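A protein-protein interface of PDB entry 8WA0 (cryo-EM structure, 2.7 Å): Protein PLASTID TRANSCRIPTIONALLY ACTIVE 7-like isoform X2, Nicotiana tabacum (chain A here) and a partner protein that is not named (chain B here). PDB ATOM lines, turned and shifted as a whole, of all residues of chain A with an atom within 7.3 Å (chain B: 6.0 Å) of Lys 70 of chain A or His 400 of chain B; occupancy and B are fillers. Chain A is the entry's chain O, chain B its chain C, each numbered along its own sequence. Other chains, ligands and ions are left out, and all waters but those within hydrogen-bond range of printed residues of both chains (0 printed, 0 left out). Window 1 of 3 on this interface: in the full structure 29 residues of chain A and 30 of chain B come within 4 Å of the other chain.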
ATOM      1  N   GLN A  61      -0.464 -11.229 -10.887  1.00  0.00           N
ATOM      2  CA  GLN A  61       0.289 -10.196 -11.547  1.00  0.00           C
ATOM      3  C   GLN A  61      -0.579  -9.007 -11.892  1.00  0.00           C
ATOM      4  O   GLN A  61      -0.186  -7.884 -11.629  1.00  0.00           O
ATOM      5  CB  GLN A  61       0.981 -10.796 -12.747  1.00  0.00           C
ATOM      6  CG  GLN A  61       1.561  -9.799 -13.721  1.00  0.00           C
ATOM      7  CD  GLN A  61       2.229 -10.498 -14.871  1.00  0.00           C
ATOM      8  OE1 GLN A  61       2.741 -11.597 -14.715  1.00  0.00           O
ATOM      9  NE2 GLN A  61       2.227  -9.869 -16.033  1.00  0.00           N
ATOM     10  N   LYS A  64      -1.393  -7.080  -8.732  1.00  0.00           N
ATOM     11  CA  LYS A  64      -0.247  -6.364  -8.243  1.00  0.00           C
ATOM     12  C   LYS A  64       0.059  -5.153  -9.088  1.00  0.00           C
ATOM     13  O   LYS A  64       0.438  -4.128  -8.559  1.00  0.00           O
ATOM     14  CB  LYS A  64       0.954  -7.290  -8.152  1.00  0.00           C
ATOM     15  CG  LYS A  64       1.981  -6.873  -7.118  1.00  0.00           C
ATOM     16  CD  LYS A  64       1.326  -6.637  -5.767  1.00  0.00           C
ATOM     17  CE  LYS A  64       0.763  -7.920  -5.178  1.00  0.00           C
ATOM     18  NZ  LYS A  64      -0.097  -7.641  -3.998  1.00  0.00           N
ATOM     19  N   ILE A  65      -0.102  -5.242 -10.397  1.00  0.00           N
ATOM     20  CA  ILE A  65       0.264  -4.113 -11.215  1.00  0.00           C
ATOM     21  C   ILE A  65      -0.612  -2.944 -10.822  1.00  0.00           C
ATOM     22  O   ILE A  65      -0.120  -1.842 -10.634  1.00  0.00           O
ATOM     23  CB  ILE A  65       0.121  -4.417 -12.709  1.00  0.00           C
ATOM     24  CG1 ILE A  65       1.182  -5.417 -13.149  1.00  0.00           C
ATOM     25  CG2 ILE A  65       0.264  -3.153 -13.539  1.00  0.00           C
ATOM     26  CD1 ILE A  65       1.018  -5.874 -14.577  1.00  0.00           C
ATOM     27  N   ARG A  66      -1.904  -3.177 -10.647  1.00  0.00           N
ATOM     28  CA  ARG A  66      -2.782  -2.111 -10.219  1.00  0.00           C
ATOM     29  C   ARG A  66      -2.486  -1.613  -8.830  1.00  0.00           C
ATOM     30  O   ARG A  66      -2.451  -0.416  -8.591  1.00  0.00           O
ATOM     31  CB  ARG A  66      -4.222  -2.565 -10.293  1.00  0.00           C
ATOM     32  CG  ARG A  66      -4.618  -3.120 -11.647  1.00  0.00           C
ATOM     33  CD  ARG A  66      -6.121  -3.316 -11.724  1.00  0.00           C
ATOM     34  NE  ARG A  66      -6.657  -3.861 -10.480  1.00  0.00           N
ATOM     35  CZ  ARG A  66      -6.890  -5.151 -10.262  1.00  0.00           C
ATOM     36  NH1 ARG A  66      -6.647  -6.044 -11.211  1.00  0.00           N
ATOM     37  NH2 ARG A  66      -7.376  -5.547  -9.094  1.00  0.00           N
ATOM     38  N   ASP A  67      -2.274  -2.525  -7.903  1.00  0.00           N
ATOM     39  CA  ASP A  67      -1.979  -2.153  -6.529  1.00  0.00           C
ATOM     40  C   ASP A  67      -0.645  -1.462  -6.335  1.00  0.00           C
ATOM     41  O   ASP A  67      -0.540  -0.516  -5.568  1.00  0.00           O
ATOM     42  CB  ASP A  67      -2.051  -3.387  -5.648  1.00  0.00           C
ATOM     43  CG  ASP A  67      -2.096  -3.054  -4.179  1.00  0.00           C
ATOM     44  OD1 ASP A  67      -2.604  -1.970  -3.827  1.00  0.00           O
ATOM     45  OD2 ASP A  67      -1.636  -3.886  -3.370  1.00  0.00           O
ATOM     46  N   GLY A  68       0.383  -1.917  -7.023  1.00  0.00           N
ATOM     47  CA  GLY A  68       1.713  -1.371  -6.851  1.00  0.00           C
ATOM     48  C   GLY A  68       1.900   0.067  -7.218  1.00  0.00           C
ATOM     49  O   GLY A  68       2.734   0.741  -6.637  1.00  0.00           O
ATOM     50  N   GLY A  69       1.143   0.554  -8.181  1.00  0.00           N
ATOM     51  CA  GLY A  69       1.362   1.901  -8.649  1.00  0.00           C
ATOM     52  C   GLY A  69       2.052   1.901  -9.978  1.00  0.00           C
ATOM     53  O   GLY A  69       2.491   2.937 -10.451  1.00  0.00           O
ATOM     54  N   LYS A  70       2.181   0.735 -10.580  1.00  0.00           N
ATOM     55  CA  LYS A  70       2.744   0.661 -11.907  1.00  0.00           C
ATOM     56  C   LYS A  70       1.798   1.252 -12.935  1.00  0.00           C
ATOM     57  O   LYS A  70       2.216   1.605 -14.017  1.00  0.00           O
ATOM     58  CB  LYS A  70       3.106  -0.767 -12.249  1.00  0.00           C
ATOM     59  CG  LYS A  70       3.999  -1.426 -11.218  1.00  0.00           C
ATOM     60  CD  LYS A  70       4.516  -2.762 -11.715  1.00  0.00           C
ATOM     61  CE  LYS A  70       5.372  -2.584 -12.954  1.00  0.00           C
ATOM     62  NZ  LYS A  70       6.580  -1.758 -12.687  1.00  0.00           N
ATOM     63  N   LEU A  71       0.519   1.356 -12.607  1.00  0.00           N
ATOM     64  CA  LEU A  71      -0.444   1.912 -13.528  1.00  0.00           C
ATOM     65  C   LEU A  71      -0.065   3.328 -13.845  1.00  0.00           C
ATOM     66  O   LEU A  71      -0.162   3.755 -14.981  1.00  0.00           O
ATOM     67  CB  LEU A  71      -1.838   1.914 -12.936  1.00  0.00           C
ATOM     68  CG  LEU A  71      -2.706   0.666 -12.903  1.00  0.00           C
ATOM     69  CD1 LEU A  71      -4.053   1.041 -12.316  1.00  0.00           C
ATOM     70  CD2 LEU A  71      -2.889   0.107 -14.299  1.00  0.00           C
ATOM     71  N   LEU A  72       0.383   4.068 -12.851  1.00  0.00           N
ATOM     72  CA  LEU A  72       0.729   5.445 -13.076  1.00  0.00           C
ATOM     73  C   LEU A  72       1.855   5.540 -14.071  1.00  0.00           C
ATOM     74  O   LEU A  72       1.832   6.381 -14.950  1.00  0.00           O
ATOM     75  CB  LEU A  72       1.113   6.124 -11.782  1.00  0.00           C
ATOM     76  CG  LEU A  72       1.518   7.591 -11.795  1.00  0.00           C
ATOM     77  CD1 LEU A  72       0.400   8.451 -12.347  1.00  0.00           C
ATOM     78  CD2 LEU A  72       1.872   8.013 -10.383  1.00  0.00           C
ATOM     79  N   THR A  73       2.834   4.664 -13.970  1.00  0.00           N
ATOM     80  CA  THR A  73       3.963   4.728 -14.862  1.00  0.00           C
ATOM     81  C   THR A  73       3.537   4.515 -16.291  1.00  0.00           C
ATOM     82  O   THR A  73       4.007   5.199 -17.177  1.00  0.00           O
ATOM     83  CB  THR A  73       5.014   3.690 -14.505  1.00  0.00           C
ATOM     84  OG1 THR A  73       4.613   2.406 -14.987  1.00  0.00           O
ATOM     85  CG2 THR A  73       5.213   3.633 -13.007  1.00  0.00           C
ATOM     86  N   MET A  74       2.632   3.583 -16.524  1.00  0.00           N
ATOM     87  CA  MET A  74       2.157   3.318 -17.866  1.00  0.00           C
ATOM     88  C   MET A  74       1.452   4.519 -18.413  1.00  0.00           C
ATOM     89  O   MET A  74       1.558   4.826 -19.589  1.00  0.00           O
ATOM     90  CB  MET A  74       1.188   2.160 -17.870  1.00  0.00           C
ATOM     91  CG  MET A  74       1.714   0.901 -17.217  1.00  0.00           C
ATOM     92  SD  MET A  74       0.502  -0.424 -17.326  1.00  0.00           S
ATOM     93  CE  MET A  74      -0.993   0.549 -17.303  1.00  0.00           C
ATOM     94  N   ASP A  75       0.687   5.180 -17.571  1.00  0.00           N
ATOM     95  CA  ASP A  75      -0.044   6.341 -18.009  1.00  0.00           C
ATOM     96  C   ASP A  75       0.833   7.493 -18.429  1.00  0.00           C
ATOM     97  O   ASP A  75       0.563   8.123 -19.431  1.00  0.00           O
ATOM     98  CB  ASP A  75      -1.012   6.759 -16.930  1.00  0.00           C
ATOM     99  CG  ASP A  75      -2.033   5.684 -16.634  1.00  0.00           C
ATOM    100  OD1 ASP A  75      -2.117   4.718 -17.416  1.00  0.00           O
ATOM    101  OD2 ASP A  75      -2.753   5.793 -15.629  1.00  0.00           O
ATOM    102  N   ILE A  76       1.891   7.766 -17.688  1.00  0.00           N
ATOM    103  CA  ILE A  76       2.746   8.881 -18.016  1.00  0.00           C
ATOM    104  C   ILE A  76       3.268   8.675 -19.418  1.00  0.00           C
ATOM    105  O   ILE A  76       3.257   9.595 -20.217  1.00  0.00           O
ATOM    106  CB  ILE A  76       3.858   9.048 -16.986  1.00  0.00           C
ATOM    107  CG1 ILE A  76       3.252   9.366 -15.624  1.00  0.00           C
ATOM    108  CG2 ILE A  76       4.815  10.151 -17.393  1.00  0.00           C
ATOM    109  CD1 ILE A  76       4.270   9.453 -14.514  1.00  0.00           C
ATOM    110  N   SER B 398      10.075  -2.987  -5.969  1.00  0.00           N
ATOM    111  CA  SER B 398       9.911  -2.750  -7.396  1.00  0.00           C
ATOM    112  C   SER B 398      10.816  -1.635  -7.842  1.00  0.00           C
ATOM    113  O   SER B 398      11.393  -0.956  -7.020  1.00  0.00           O
ATOM    114  CB  SER B 398       8.482  -2.378  -7.702  1.00  0.00           C
ATOM    115  OG  SER B 398       7.591  -3.316  -7.137  1.00  0.00           O
ATOM    116  N   LEU B 399      10.933  -1.421  -9.139  1.00  0.00           N
ATOM    117  CA  LEU B 399      11.860  -0.419  -9.659  1.00  0.00           C
ATOM    118  C   LEU B 399      11.551   1.010  -9.255  1.00  0.00           C
ATOM    119  O   LEU B 399      12.450   1.818  -9.123  1.00  0.00           O
ATOM    120  CB  LEU B 399      11.952  -0.529 -11.172  1.00  0.00           C
ATOM    121  CG  LEU B 399      13.195  -0.018 -11.892  1.00  0.00           C
ATOM    122  CD1 LEU B 399      14.425  -0.758 -11.401  1.00  0.00           C
ATOM    123  CD2 LEU B 399      13.028  -0.216 -13.387  1.00  0.00           C
ATOM    124  N   HIS B 400      10.288   1.343  -9.085  1.00  0.00           N
ATOM    125  CA  HIS B 400       9.899   2.694  -8.745  1.00  0.00           C
ATOM    126  C   HIS B 400       9.874   2.976  -7.263  1.00  0.00           C
ATOM    127  O   HIS B 400       9.498   4.060  -6.865  1.00  0.00           O
ATOM    128  CB  HIS B 400       8.535   3.003  -9.345  1.00  0.00           C
ATOM    129  CG  HIS B 400       7.422   2.162  -8.810  1.00  0.00           C
ATOM    130  ND1 HIS B 400       7.219   0.858  -9.201  1.00  0.00           N
ATOM    131  CD2 HIS B 400       6.427   2.452  -7.940  1.00  0.00           C
ATOM    132  CE1 HIS B 400       6.160   0.373  -8.577  1.00  0.00           C
ATOM    133  NE2 HIS B 400       5.662   1.320  -7.806  1.00  0.00           N
ATOM    134  N   ARG B 401      10.257   2.025  -6.432  1.00  0.00           N
ATOM    135  CA  ARG B 401      10.147   2.211  -4.999  1.00  0.00           C
ATOM    136  C   ARG B 401      11.441   2.109  -4.230  1.00  0.00           C
ATOM    137  O   ARG B 401      12.394   1.519  -4.704  1.00  0.00           O
ATOM    138  CB  ARG B 401       9.171   1.201  -4.430  1.00  0.00           C
ATOM    139  CG  ARG B 401       7.715   1.505  -4.677  1.00  0.00           C
ATOM    140  CD  ARG B 401       6.871   0.392  -4.098  1.00  0.00           C
ATOM    141  NE  ARG B 401       5.502   0.818  -3.855  1.00  0.00           N
ATOM    142  CZ  ARG B 401       4.612   0.089  -3.195  1.00  0.00           C
ATOM    143  NH1 ARG B 401       4.957  -1.095  -2.714  1.00  0.00           N
ATOM    144  NH2 ARG B 401       3.384   0.544  -3.010  1.00  0.00           N
ATOM    145  N   CYS B 402      11.494   2.725  -3.058  1.00  0.00           N
ATOM    146  CA  CYS B 402      12.668   2.644  -2.201  1.00  0.00           C
ATOM    147  C   CYS B 402      12.181   2.534  -0.777  1.00  0.00           C
ATOM    148  O   CYS B 402      11.049   2.869  -0.494  1.00  0.00           O
ATOM    149  CB  CYS B 402      13.549   3.871  -2.343  1.00  0.00           C
ATOM    150  SG  CYS B 402      13.077   5.306  -1.369  1.00  0.00           S
ATOM    151  N   ALA B 472      15.083   9.397  -8.664  1.00  0.00           N
ATOM    152  CA  ALA B 472      13.956   9.599  -7.762  1.00  0.00           C
ATOM    153  C   ALA B 472      13.087   8.392  -7.551  1.00  0.00           C
ATOM    154  O   ALA B 472      12.859   7.637  -8.477  1.00  0.00           O
ATOM    155  CB  ALA B 472      13.118  10.735  -8.245  1.00  0.00           C
ATOM    156  N   PHE B 473      12.575   8.213  -6.340  1.00  0.00           N
ATOM    157  CA  PHE B 473      11.788   7.037  -6.020  1.00  0.00           C
ATOM    158  C   PHE B 473      10.594   7.354  -5.160  1.00  0.00           C
ATOM    159  O   PHE B 473      10.524   8.421  -4.597  1.00  0.00           O
ATOM    160  CB  PHE B 473      12.652   6.057  -5.264  1.00  0.00           C
ATOM    161  CG  PHE B 473      13.852   5.579  -6.016  1.00  0.00           C
ATOM    162  CD1 PHE B 473      13.742   4.561  -6.935  1.00  0.00           C
ATOM    163  CD2 PHE B 473      15.096   6.127  -5.777  1.00  0.00           C
ATOM    164  CE1 PHE B 473      14.846   4.113  -7.622  1.00  0.00           C
ATOM    165  CE2 PHE B 473      16.205   5.686  -6.460  1.00  0.00           C
ATOM    166  CZ  PHE B 473      16.079   4.677  -7.385  1.00  0.00           C
ATOM    167  N   GLN B 474       9.660   6.424  -5.035  1.00  0.00           N
ATOM    168  CA  GLN B 474       8.507   6.615  -4.173  1.00  0.00           C
ATOM    169  C   GLN B 474       8.837   5.935  -2.891  1.00  0.00           C
ATOM    170  O   GLN B 474       9.107   4.753  -2.876  1.00  0.00           O
ATOM    171  CB  GLN B 474       7.290   5.936  -4.752  1.00  0.00           C
ATOM    172  CG  GLN B 474       6.019   6.746  -4.652  1.00  0.00           C
ATOM    173  CD  GLN B 474       5.574   6.932  -3.227  1.00  0.00           C
ATOM    174  OE1 GLN B 474       5.390   5.969  -2.493  1.00  0.00           O
ATOM    175  NE2 GLN B 474       5.396   8.176  -2.827  1.00  0.00           N
ATOM    176  N   PRO B 475       8.803   6.664  -1.790  1.00  0.00           N
ATOM    177  CA  PRO B 475       9.243   6.057  -0.548  1.00  0.00           C
ATOM    178  C   PRO B 475       8.293   5.096   0.123  1.00  0.00           C
ATOM    179  O   PRO B 475       7.100   5.346   0.124  1.00  0.00           O
ATOM    180  CB  PRO B 475       9.471   7.262   0.339  1.00  0.00           C
ATOM    181  CG  PRO B 475       8.624   8.342  -0.219  1.00  0.00           C
ATOM    182  CD  PRO B 475       8.694   8.123  -1.687  1.00  0.00           C
ATOM    183  N   PHE B 521      12.842   9.348 -12.940  1.00  0.00           N
ATOM    184  CA  PHE B 521      12.488   8.086 -12.364  1.00  0.00           C
ATOM    185  C   PHE B 521      13.142   7.073 -13.245  1.00  0.00           C
ATOM    186  O   PHE B 521      13.365   7.327 -14.400  1.00  0.00           O
ATOM    187  CB  PHE B 521      11.014   7.925 -12.375  1.00  0.00           C
ATOM    188  CG  PHE B 521      10.339   8.072 -11.050  1.00  0.00           C
ATOM    189  CD1 PHE B 521      10.333   9.269 -10.381  1.00  0.00           C
ATOM    190  CD2 PHE B 521       9.641   7.023 -10.512  1.00  0.00           C
ATOM    191  CE1 PHE B 521       9.680   9.406  -9.176  1.00  0.00           C
ATOM    192  CE2 PHE B 521       8.985   7.151  -9.312  1.00  0.00           C
ATOM    193  CZ  PHE B 521       9.002   8.344  -8.643  1.00  0.00           C
ATOM    194  N   SER B 522      13.459   5.915 -12.728  1.00  0.00           N
ATOM    195  CA  SER B 522      14.204   4.902 -13.437  1.00  0.00           C
ATOM    196  C   SER B 522      13.648   4.303 -14.662  1.00  0.00           C
ATOM    197  O   SER B 522      14.378   3.996 -15.579  1.00  0.00           O
ATOM    198  CB  SER B 522      14.546   3.812 -12.467  1.00  0.00           C
ATOM    199  OG  SER B 522      15.267   4.326 -11.372  1.00  0.00           O
ATOM    200  N   HIS B 523      12.375   4.100 -14.702  1.00  0.00           N
ATOM    201  CA  HIS B 523      11.743   3.598 -15.859  1.00  0.00           C
ATOM    202  C   HIS B 523      11.968   4.473 -17.051  1.00  0.00           C
ATOM    203  O   HIS B 523      12.041   3.978 -18.140  1.00  0.00           O
ATOM    204  CB  HIS B 523      10.276   3.339 -15.571  1.00  0.00           C
ATOM    205  CG  HIS B 523       9.437   4.548 -15.335  1.00  0.00           C
ATOM    206  ND1 HIS B 523       9.302   5.128 -14.097  1.00  0.00           N
ATOM    207  CD2 HIS B 523       8.617   5.235 -16.163  1.00  0.00           C
ATOM    208  CE1 HIS B 523       8.478   6.155 -14.182  1.00  0.00           C
ATOM    209  NE2 HIS B 523       8.043   6.237 -15.425  1.00  0.00           N
ATOM    210  N   PHE B 680       0.643  -6.784 -18.616  1.00  0.00           N
ATOM    211  CA  PHE B 680       0.675  -5.344 -18.674  1.00  0.00           C
ATOM    212  C   PHE B 680      -0.458  -4.876 -19.549  1.00  0.00           C
ATOM    213  O   PHE B 680      -1.097  -3.886 -19.247  1.00  0.00           O
ATOM    214  CB  PHE B 680       1.987  -4.900 -19.280  1.00  0.00           C
ATOM    215  CG  PHE B 680       2.663  -3.788 -18.548  1.00  0.00           C
ATOM    216  CD1 PHE B 680       2.777  -3.811 -17.176  1.00  0.00           C
ATOM    217  CD2 PHE B 680       3.222  -2.736 -19.244  1.00  0.00           C
ATOM    218  CE1 PHE B 680       3.416  -2.790 -16.504  1.00  0.00           C
ATOM    219  CE2 PHE B 680       3.865  -1.714 -18.582  1.00  0.00           C
ATOM    220  CZ  PHE B 680       3.965  -1.742 -17.209  1.00  0.00           C
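O of Gly 68 of chain A is in hydrogen-bond range of NE2 of His 400 of chain B (3.2 Å).
The backbone NH (N) of Gln 474 of chain B lies within hydrogen-bond range of the backbone carbonyl oxygen (O) of His 400 of chain B, at 3.0 Å. The side-chain hydroxyl of Thr 73 of chain A is in hydrogen-bond range of the backbone carbonyl oxygen of Lys 70 of chain A. The backbone carbonyl oxygen of Ile 65 of chain A sits at hydrogen-bond distance from the backbone NH of Lys 70 of chain A.
Among the printed residues, pairs that only touch across the chains: Ile 65 of chain A with Phe 680 of chain B (3.8 Å), Gly 68 of chain A with Arg 401 of chain B (3.7 Å), Lys 70 of chain A with His 400 of chain B (3.9 Å) and Met 74 of chain A with Phe 680 of chain B (3.5 Å).
Of chain B, only His 400 (3.9 Å) comes within 4 Å of Lys 70 of chain A. Of the printed residues of chain A, Arg 401 of chain B touches Gly 68 (3.7 Å). Printed residues of chain B within 4 Å of Ile 65 of chain A: Phe 680 (3.8 Å). Printed residues of chain A within 4 Å of Phe 680 of chain B: Ile 65 (3.8 Å) and Met 74 (3.5 Å). Printed residues of chain B within 4 Å of Met 74 of chain A: Phe 680. Printed residues of chain B within 4 Å of Gly 68 of chain A: His 400 (3.2 Å) and Arg 401 (3.7 Å). The nearest residue of chain A that does not touch His 400 of chain B is Gly 69 of chain A (4.3 Å). The nearest printed residue of chain B that does not touch Ile 65 of chain A is His 400 of chain B (7.0 Å).
Of the 14 printed residues of chain A, 4 touch a printed residue of chain B. Hydrophobic or aromatic side chains of chain A within 4 Å of the printed part of chain B: Ile 65 and Met 74. Of the 13 printed residues of chain B, 3 touch a printed residue of chain A. Printed residues of chain B that touch a printed residue of chain A: His 400, Arg 401 and Phe 680. Hydrophobic or aromatic side chains of chain B within 4 Å of the printed part of chain A: His 400 and Phe 680. Along chain B the printed residues that touch a printed residue of chain A span positions 400 to 680. Among the printed residues, no Asp or Glu carboxylate lies within 4 Å of a Lys or Arg side-chain nitrogen of the other chain.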
